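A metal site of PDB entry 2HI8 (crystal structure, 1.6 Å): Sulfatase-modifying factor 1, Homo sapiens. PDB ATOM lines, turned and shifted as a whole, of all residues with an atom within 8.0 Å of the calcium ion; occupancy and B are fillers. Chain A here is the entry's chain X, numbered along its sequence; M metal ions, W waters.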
ATOM      1  N   TYR A  44     -12.181   9.495  -5.636  1.00  0.00           N
ATOM      2  CA  TYR A  44     -13.327  10.064  -4.969  1.00  0.00           C
ATOM      3  C   TYR A  44     -14.515   9.105  -4.964  1.00  0.00           C
ATOM      4  O   TYR A  44     -14.687   8.294  -5.868  1.00  0.00           O
ATOM      5  CB  TYR A  44     -13.780  11.329  -5.720  1.00  0.00           C
ATOM      6  CG  TYR A  44     -12.656  12.286  -6.032  1.00  0.00           C
ATOM      7  CD1 TYR A  44     -12.041  13.010  -5.033  1.00  0.00           C
ATOM      8  CD2 TYR A  44     -12.190  12.436  -7.330  1.00  0.00           C
ATOM      9  CE1 TYR A  44     -11.014  13.880  -5.307  1.00  0.00           C
ATOM     10  CE2 TYR A  44     -11.176  13.300  -7.633  1.00  0.00           C
ATOM     11  CZ  TYR A  44     -10.591  14.039  -6.608  1.00  0.00           C
ATOM     12  OH  TYR A  44      -9.550  14.909  -6.878  1.00  0.00           O
ATOM     13  N   GLU A  45     -15.338   9.239  -3.925  1.00  0.00           N
ATOM     14  CA  GLU A  45     -16.677   8.692  -3.979  1.00  0.00           C
ATOM     15  C   GLU A  45     -17.314   9.206  -5.267  1.00  0.00           C
ATOM     16  O   GLU A  45     -17.051  10.322  -5.709  1.00  0.00           O
ATOM     17  CB  GLU A  45     -17.500   9.160  -2.798  1.00  0.00           C
ATOM     18  CG  GLU A  45     -16.976   8.650  -1.462  1.00  0.00           C
ATOM     19  CD  GLU A  45     -17.345   9.541  -0.281  1.00  0.00           C
ATOM     20  OE1 GLU A  45     -17.398  10.777  -0.452  1.00  0.00           O
ATOM     21  OE2 GLU A  45     -17.548   8.981   0.821  1.00  0.00           O
ATOM     22  N   PRO A 120     -21.098  13.151  -2.581  1.00  0.00           N
ATOM     23  CA  PRO A 120     -21.257  11.770  -3.032  1.00  0.00           C
ATOM     24  C   PRO A 120     -22.716  11.467  -3.297  1.00  0.00           C
ATOM     25  O   PRO A 120     -23.611  11.927  -2.565  1.00  0.00           O
ATOM     26  CB  PRO A 120     -20.773  10.966  -1.817  1.00  0.00           C
ATOM     27  CG  PRO A 120     -21.004  11.869  -0.672  1.00  0.00           C
ATOM     28  CD  PRO A 120     -20.629  13.217  -1.196  1.00  0.00           C
ATOM     29  N   TRP A 146     -10.555  -2.577  -1.222  1.00  0.00           N
ATOM     30  CA  TRP A 146     -11.043  -1.393  -0.555  1.00  0.00           C
ATOM     31  C   TRP A 146     -10.239  -1.137   0.727  1.00  0.00           C
ATOM     32  O   TRP A 146      -9.753  -0.011   0.951  1.00  0.00           O
ATOM     33  CB  TRP A 146     -12.545  -1.516  -0.259  1.00  0.00           C
ATOM     34  CG  TRP A 146     -13.141  -0.220   0.200  1.00  0.00           C
ATOM     35  CD1 TRP A 146     -13.852   0.660  -0.535  1.00  0.00           C
ATOM     36  CD2 TRP A 146     -12.978   0.373   1.485  1.00  0.00           C
ATOM     37  NE1 TRP A 146     -14.181   1.756   0.209  1.00  0.00           N
ATOM     38  CE2 TRP A 146     -13.667   1.601   1.464  1.00  0.00           C
ATOM     39  CE3 TRP A 146     -12.366  -0.033   2.671  1.00  0.00           C
ATOM     40  CZ2 TRP A 146     -13.714   2.431   2.564  1.00  0.00           C
ATOM     41  CZ3 TRP A 146     -12.421   0.796   3.750  1.00  0.00           C
ATOM     42  CH2 TRP A 146     -13.077   2.017   3.697  1.00  0.00           C
ATOM     43  N   ASN A 174     -14.978  13.344   7.355  1.00  0.00           N
ATOM     44  CA  ASN A 174     -16.290  13.848   7.701  1.00  0.00           C
ATOM     45  C   ASN A 174     -17.071  12.771   8.443  1.00  0.00           C
ATOM     46  O   ASN A 174     -17.596  11.842   7.843  1.00  0.00           O
ATOM     47  CB  ASN A 174     -17.023  14.291   6.455  1.00  0.00           C
ATOM     48  CG  ASN A 174     -18.411  14.789   6.735  1.00  0.00           C
ATOM     49  OD1 ASN A 174     -18.721  15.178   7.861  1.00  0.00           O
ATOM     50  ND2 ASN A 174     -19.262  14.774   5.709  1.00  0.00           N
ATOM     51  N   TYR A 207      -9.668  10.212  -1.327  1.00  0.00           N
ATOM     52  CA  TYR A 207     -10.433  11.159  -0.528  1.00  0.00           C
ATOM     53  C   TYR A 207     -11.646  10.472   0.079  1.00  0.00           C
ATOM     54  O   TYR A 207     -12.327   9.721  -0.599  1.00  0.00           O
ATOM     55  CB  TYR A 207     -10.885  12.307  -1.427  1.00  0.00           C
ATOM     56  CG  TYR A 207      -9.744  13.131  -1.916  1.00  0.00           C
ATOM     57  CD1 TYR A 207      -8.941  12.686  -2.960  1.00  0.00           C
ATOM     58  CD2 TYR A 207      -9.414  14.341  -1.293  1.00  0.00           C
ATOM     59  CE1 TYR A 207      -7.858  13.415  -3.392  1.00  0.00           C
ATOM     60  CE2 TYR A 207      -8.340  15.091  -1.719  1.00  0.00           C
ATOM     61  CZ  TYR A 207      -7.579  14.622  -2.773  1.00  0.00           C
ATOM     62  OH  TYR A 207      -6.502  15.369  -3.185  1.00  0.00           O
ATOM     63  N   ASN A 208     -11.882  10.742   1.361  1.00  0.00           N
ATOM     64  CA  ASN A 208     -13.112  10.370   2.063  1.00  0.00           C
ATOM     65  C   ASN A 208     -13.347   8.883   2.029  1.00  0.00           C
ATOM     66  O   ASN A 208     -14.467   8.428   1.970  1.00  0.00           O
ATOM     67  CB  ASN A 208     -14.294  11.149   1.515  1.00  0.00           C
ATOM     68  CG  ASN A 208     -14.111  12.609   1.710  1.00  0.00           C
ATOM     69  OD1 ASN A 208     -14.031  13.060   2.853  1.00  0.00           O
ATOM     70  ND2 ASN A 208     -13.946  13.348   0.624  1.00  0.00           N
ATOM     71  N   ILE A 209     -12.259   8.130   2.083  1.00  0.00           N
ATOM     72  CA  ILE A 209     -12.360   6.692   2.075  1.00  0.00           C
ATOM     73  C   ILE A 209     -12.931   6.260   3.426  1.00  0.00           C
ATOM     74  O   ILE A 209     -13.738   5.332   3.471  1.00  0.00           O
ATOM     75  CB  ILE A 209     -11.030   6.016   1.683  1.00  0.00           C
ATOM     76  CG1 ILE A 209     -11.218   4.510   1.478  1.00  0.00           C
ATOM     77  CG2 ILE A 209      -9.947   6.299   2.700  1.00  0.00           C
ATOM     78  CD1 ILE A 209     -11.593   4.114   0.102  1.00  0.00           C
ATOM     79  N   VAL A 210     -12.572   6.937   4.523  1.00  0.00           N
ATOM     80  CA  VAL A 210     -13.388   6.801   5.733  1.00  0.00           C
ATOM     81  C   VAL A 210     -14.224   8.068   5.874  1.00  0.00           C
ATOM     82  O   VAL A 210     -13.816   9.168   5.462  1.00  0.00           O
ATOM     83  CB  VAL A 210     -12.638   6.483   7.028  1.00  0.00           C
ATOM     84  CG1 VAL A 210     -11.893   5.179   6.892  1.00  0.00           C
ATOM     85  CG2 VAL A 210     -11.679   7.612   7.422  1.00  0.00           C
ATOM     86  N   GLY A 211     -15.428   7.889   6.416  1.00  0.00           N
ATOM     87  CA  GLY A 211     -16.391   8.966   6.570  1.00  0.00           C
ATOM     88  C   GLY A 211     -17.065   9.395   5.277  1.00  0.00           C
ATOM     89  O   GLY A 211     -16.850   8.826   4.202  1.00  0.00           O
ATOM     90  N   ASN A 212     -17.897  10.420   5.410  1.00  0.00           N
ATOM     91  CA  ASN A 212     -18.687  10.980   4.324  1.00  0.00           C
ATOM     92  C   ASN A 212     -19.797  10.023   3.947  1.00  0.00           C
ATOM     93  O   ASN A 212     -20.780   9.949   4.666  1.00  0.00           O
ATOM     94  CB  ASN A 212     -17.815  11.452   3.146  1.00  0.00           C
ATOM     95  CG  ASN A 212     -18.341  12.724   2.511  1.00  0.00           C
ATOM     96  OD1 ASN A 212     -18.919  13.572   3.184  1.00  0.00           O
ATOM     97  ND2 ASN A 212     -18.135  12.881   1.213  1.00  0.00           N
ATOM     98  N   ALA A 213     -19.668   9.267   2.854  1.00  0.00           N
ATOM     99  CA  ALA A 213     -20.622   8.196   2.585  1.00  0.00           C
ATOM    100  C   ALA A 213     -19.954   6.868   2.870  1.00  0.00           C
ATOM    101  O   ALA A 213     -18.750   6.678   2.603  1.00  0.00           O
ATOM    102  CB  ALA A 213     -21.110   8.249   1.129  1.00  0.00           C
ATOM    103  N   TRP A 214     -20.725   5.930   3.426  1.00  0.00           N
ATOM    104  CA  TRP A 214     -20.366   4.525   3.375  1.00  0.00           C
ATOM    105  C   TRP A 214     -20.127   4.105   1.936  1.00  0.00           C
ATOM    106  O   TRP A 214     -20.679   4.692   1.034  1.00  0.00           O
ATOM    107  CB  TRP A 214     -21.510   3.669   3.872  1.00  0.00           C
ATOM    108  CG  TRP A 214     -21.592   3.488   5.315  1.00  0.00           C
ATOM    109  CD1 TRP A 214     -22.399   4.171   6.178  1.00  0.00           C
ATOM    110  CD2 TRP A 214     -20.899   2.522   6.099  1.00  0.00           C
ATOM    111  NE1 TRP A 214     -22.228   3.706   7.465  1.00  0.00           N
ATOM    112  CE2 TRP A 214     -21.298   2.700   7.441  1.00  0.00           C
ATOM    113  CE3 TRP A 214     -19.952   1.537   5.793  1.00  0.00           C
ATOM    114  CZ2 TRP A 214     -20.799   1.916   8.470  1.00  0.00           C
ATOM    115  CZ3 TRP A 214     -19.447   0.782   6.829  1.00  0.00           C
ATOM    116  CH2 TRP A 214     -19.878   0.967   8.134  1.00  0.00           C
ATOM    117  N   GLU A 215     -19.343   3.058   1.741  1.00  0.00           N
ATOM    118  CA  GLU A 215     -19.008   2.620   0.396  1.00  0.00           C
ATOM    119  C   GLU A 215     -19.237   1.137   0.205  1.00  0.00           C
ATOM    120  O   GLU A 215     -18.681   0.319   0.915  1.00  0.00           O
ATOM    121  CB  GLU A 215     -17.568   2.995   0.101  1.00  0.00           C
ATOM    122  CG  GLU A 215     -17.408   4.482   0.257  1.00  0.00           C
ATOM    123  CD  GLU A 215     -16.027   4.983   0.037  1.00  0.00           C
ATOM    124  OE1 GLU A 215     -15.189   4.245  -0.490  1.00  0.00           O
ATOM    125  OE2 GLU A 215     -15.801   6.151   0.405  1.00  0.00           O
ATOM    126  N   LYS A 245     -18.056  -0.433   3.564  1.00  0.00           N
ATOM    127  CA  LYS A 245     -16.910  -0.055   4.343  1.00  0.00           C
ATOM    128  C   LYS A 245     -16.855   1.437   4.568  1.00  0.00           C
ATOM    129  O   LYS A 245     -17.429   2.228   3.818  1.00  0.00           O
ATOM    130  CB  LYS A 245     -15.620  -0.455   3.610  1.00  0.00           C
ATOM    131  CG  LYS A 245     -15.437  -1.974   3.384  1.00  0.00           C
ATOM    132  CD  LYS A 245     -15.007  -2.699   4.630  1.00  0.00           C
ATOM    133  CE  LYS A 245     -13.495  -2.727   4.758  1.00  0.00           C
ATOM    134  NZ  LYS A 245     -13.034  -3.531   5.948  1.00  0.00           N
ATOM    135  N   GLY A 246     -16.175   1.799   5.643  1.00  0.00           N
ATOM    136  CA  GLY A 246     -15.600   3.112   5.788  1.00  0.00           C
ATOM    137  C   GLY A 246     -16.338   4.100   6.666  1.00  0.00           C
ATOM    138  O   GLY A 246     -15.777   5.154   6.975  1.00  0.00           O
ATOM    139  N   GLY A 247     -17.582   3.804   7.047  1.00  0.00           N
ATOM    140  CA  GLY A 247     -18.325   4.746   7.848  1.00  0.00           C
ATOM    141  C   GLY A 247     -18.778   5.928   7.024  1.00  0.00           C
ATOM    142  O   GLY A 247     -18.573   5.985   5.814  1.00  0.00           O
ATOM    143  N   SER A 248     -19.390   6.877   7.715  1.00  0.00           N
ATOM    144  CA  SER A 248     -20.055   7.983   7.085  1.00  0.00           C
ATOM    145  C   SER A 248     -20.017   9.192   7.968  1.00  0.00           C
ATOM    146  O   SER A 248     -19.476   9.177   9.079  1.00  0.00           O
ATOM    147  CB  SER A 248     -21.528   7.633   6.789  1.00  0.00           C
ATOM    148  OG  SER A 248     -22.341   7.734   7.937  1.00  0.00           O
ATOM    149  N   TYR A 249     -20.616  10.238   7.450  1.00  0.00           N
ATOM    150  CA  TYR A 249     -20.809  11.478   8.176  1.00  0.00           C
ATOM    151  C   TYR A 249     -21.605  11.329   9.460  1.00  0.00           C
ATOM    152  O   TYR A 249     -21.601  12.232  10.291  1.00  0.00           O
ATOM    153  CB  TYR A 249     -21.431  12.516   7.244  1.00  0.00           C
ATOM    154  CG  TYR A 249     -22.898  12.318   6.894  1.00  0.00           C
ATOM    155  CD1 TYR A 249     -23.878  12.706   7.770  1.00  0.00           C
ATOM    156  CD2 TYR A 249     -23.280  11.804   5.648  1.00  0.00           C
ATOM    157  CE1 TYR A 249     -25.221  12.554   7.456  1.00  0.00           C
ATOM    158  CE2 TYR A 249     -24.626  11.655   5.320  1.00  0.00           C
ATOM    159  CZ  TYR A 249     -25.580  12.024   6.230  1.00  0.00           C
ATOM    160  OH  TYR A 249     -26.926  11.905   5.925  1.00  0.00           O
ATOM    161  N   ASN A 275     -26.762   7.724   3.809  1.00  0.00           N
ATOM    162  CA  ASN A 275     -25.375   7.750   4.208  1.00  0.00           C
ATOM    163  C   ASN A 275     -24.515   6.766   3.461  1.00  0.00           C
ATOM    164  O   ASN A 275     -23.411   6.450   3.908  1.00  0.00           O
ATOM    165  CB  ASN A 275     -25.241   7.548   5.716  1.00  0.00           C
ATOM    166  CG  ASN A 275     -25.583   6.140   6.158  1.00  0.00           C
ATOM    167  OD1 ASN A 275     -26.128   5.364   5.399  1.00  0.00           O
ATOM    168  ND2 ASN A 275     -25.213   5.799   7.407  1.00  0.00           N
ATOM    169  N   GLY A 277     -22.979   5.329  -0.249  1.00  0.00           N
ATOM    170  CA  GLY A 277     -22.618   5.559  -1.631  1.00  0.00           C
ATOM    171  C   GLY A 277     -21.591   4.535  -2.024  1.00  0.00           C
ATOM    172  O   GLY A 277     -21.651   3.386  -1.568  1.00  0.00           O
ATOM    173  N   PHE A 278     -20.652   4.947  -2.859  1.00  0.00           N
ATOM    174  CA  PHE A 278     -19.647   4.023  -3.365  1.00  0.00           C
ATOM    175  C   PHE A 278     -18.589   4.707  -4.161  1.00  0.00           C
ATOM    176  O   PHE A 278     -18.759   5.848  -4.574  1.00  0.00           O
ATOM    177  CB  PHE A 278     -20.296   2.941  -4.235  1.00  0.00           C
ATOM    178  CG  PHE A 278     -20.871   3.460  -5.528  1.00  0.00           C
ATOM    179  CD1 PHE A 278     -22.089   4.138  -5.556  1.00  0.00           C
ATOM    180  CD2 PHE A 278     -20.201   3.243  -6.724  1.00  0.00           C
ATOM    181  CE1 PHE A 278     -22.607   4.612  -6.754  1.00  0.00           C
ATOM    182  CE2 PHE A 278     -20.737   3.713  -7.934  1.00  0.00           C
ATOM    183  CZ  PHE A 278     -21.929   4.413  -7.925  1.00  0.00           C
ATOM    184  N   ARG A 279     -17.516   3.981  -4.424  1.00  0.00           N
ATOM    185  CA  ARG A 279     -16.560   4.354  -5.452  1.00  0.00           C
ATOM    186  C   ARG A 279     -16.236   3.108  -6.239  1.00  0.00           C
ATOM    187  O   ARG A 279     -16.466   1.996  -5.780  1.00  0.00           O
ATOM    188  CB  ARG A 279     -15.298   4.931  -4.859  1.00  0.00           C
ATOM    189  CG  ARG A 279     -14.373   3.921  -4.197  1.00  0.00           C
ATOM    190  CD  ARG A 279     -13.159   4.633  -3.583  1.00  0.00           C
ATOM    191  NE  ARG A 279     -13.554   5.425  -2.420  1.00  0.00           N
ATOM    192  CZ  ARG A 279     -13.115   6.628  -2.114  1.00  0.00           C
ATOM    193  NH1 ARG A 279     -12.215   7.253  -2.859  1.00  0.00           N
ATOM    194  NH2 ARG A 279     -13.565   7.221  -1.026  1.00  0.00           N
HETATM  195 CA    CA M   1     -16.557   7.447   2.212  1.00  0.00          CA
HETATM  196  O   HOH W   1     -16.336   5.803   3.773  1.00  0.00           O
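The side-chain amide nitrogen (ND2) of Asn 212 sits at hydrogen-bond distance from the side-chain carboxylate (OE1) of Glu 45 (2.8 Å).
The side-chain carboxylate of Glu 215 sits at hydrogen-bond distance from the indole nitrogen of Trp 146 (2.8 Å).
NE of Arg 279 lies within salt-bridge range of OE1 of Glu 215 (2.8 Å).
O of Gly 246 sits at hydrogen-bond distance from N of Gly 211 (2.8 Å).
O of Asn 208 lies close to NH2 of Arg 279, 3.4 Å away.
O of Glu 215 is in hydrogen-bond range of N of Lys 245 (2.8 Å).
Residues that only touch the calcium ion: Ile 209.
Within 4 Å of the calcium ion: Glu 45, Asn 208, Ile 209, Gly 211, Ala 213 and Glu 215.
Water W1 is bound to the calcium ion.
The side-chain carboxylate (OE2) of Glu 45 binds the calcium ion.
The calcium ion is bound by O of Asn 208 (2.3 Å).
OE2 of Glu 215 is bound to the calcium ion, at 2.3 Å.
The calcium ion is bound by the backbone carbonyl oxygen (O) of Ala 213, 2.4 Å away.
O of Gly 211 binds the calcium ion.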
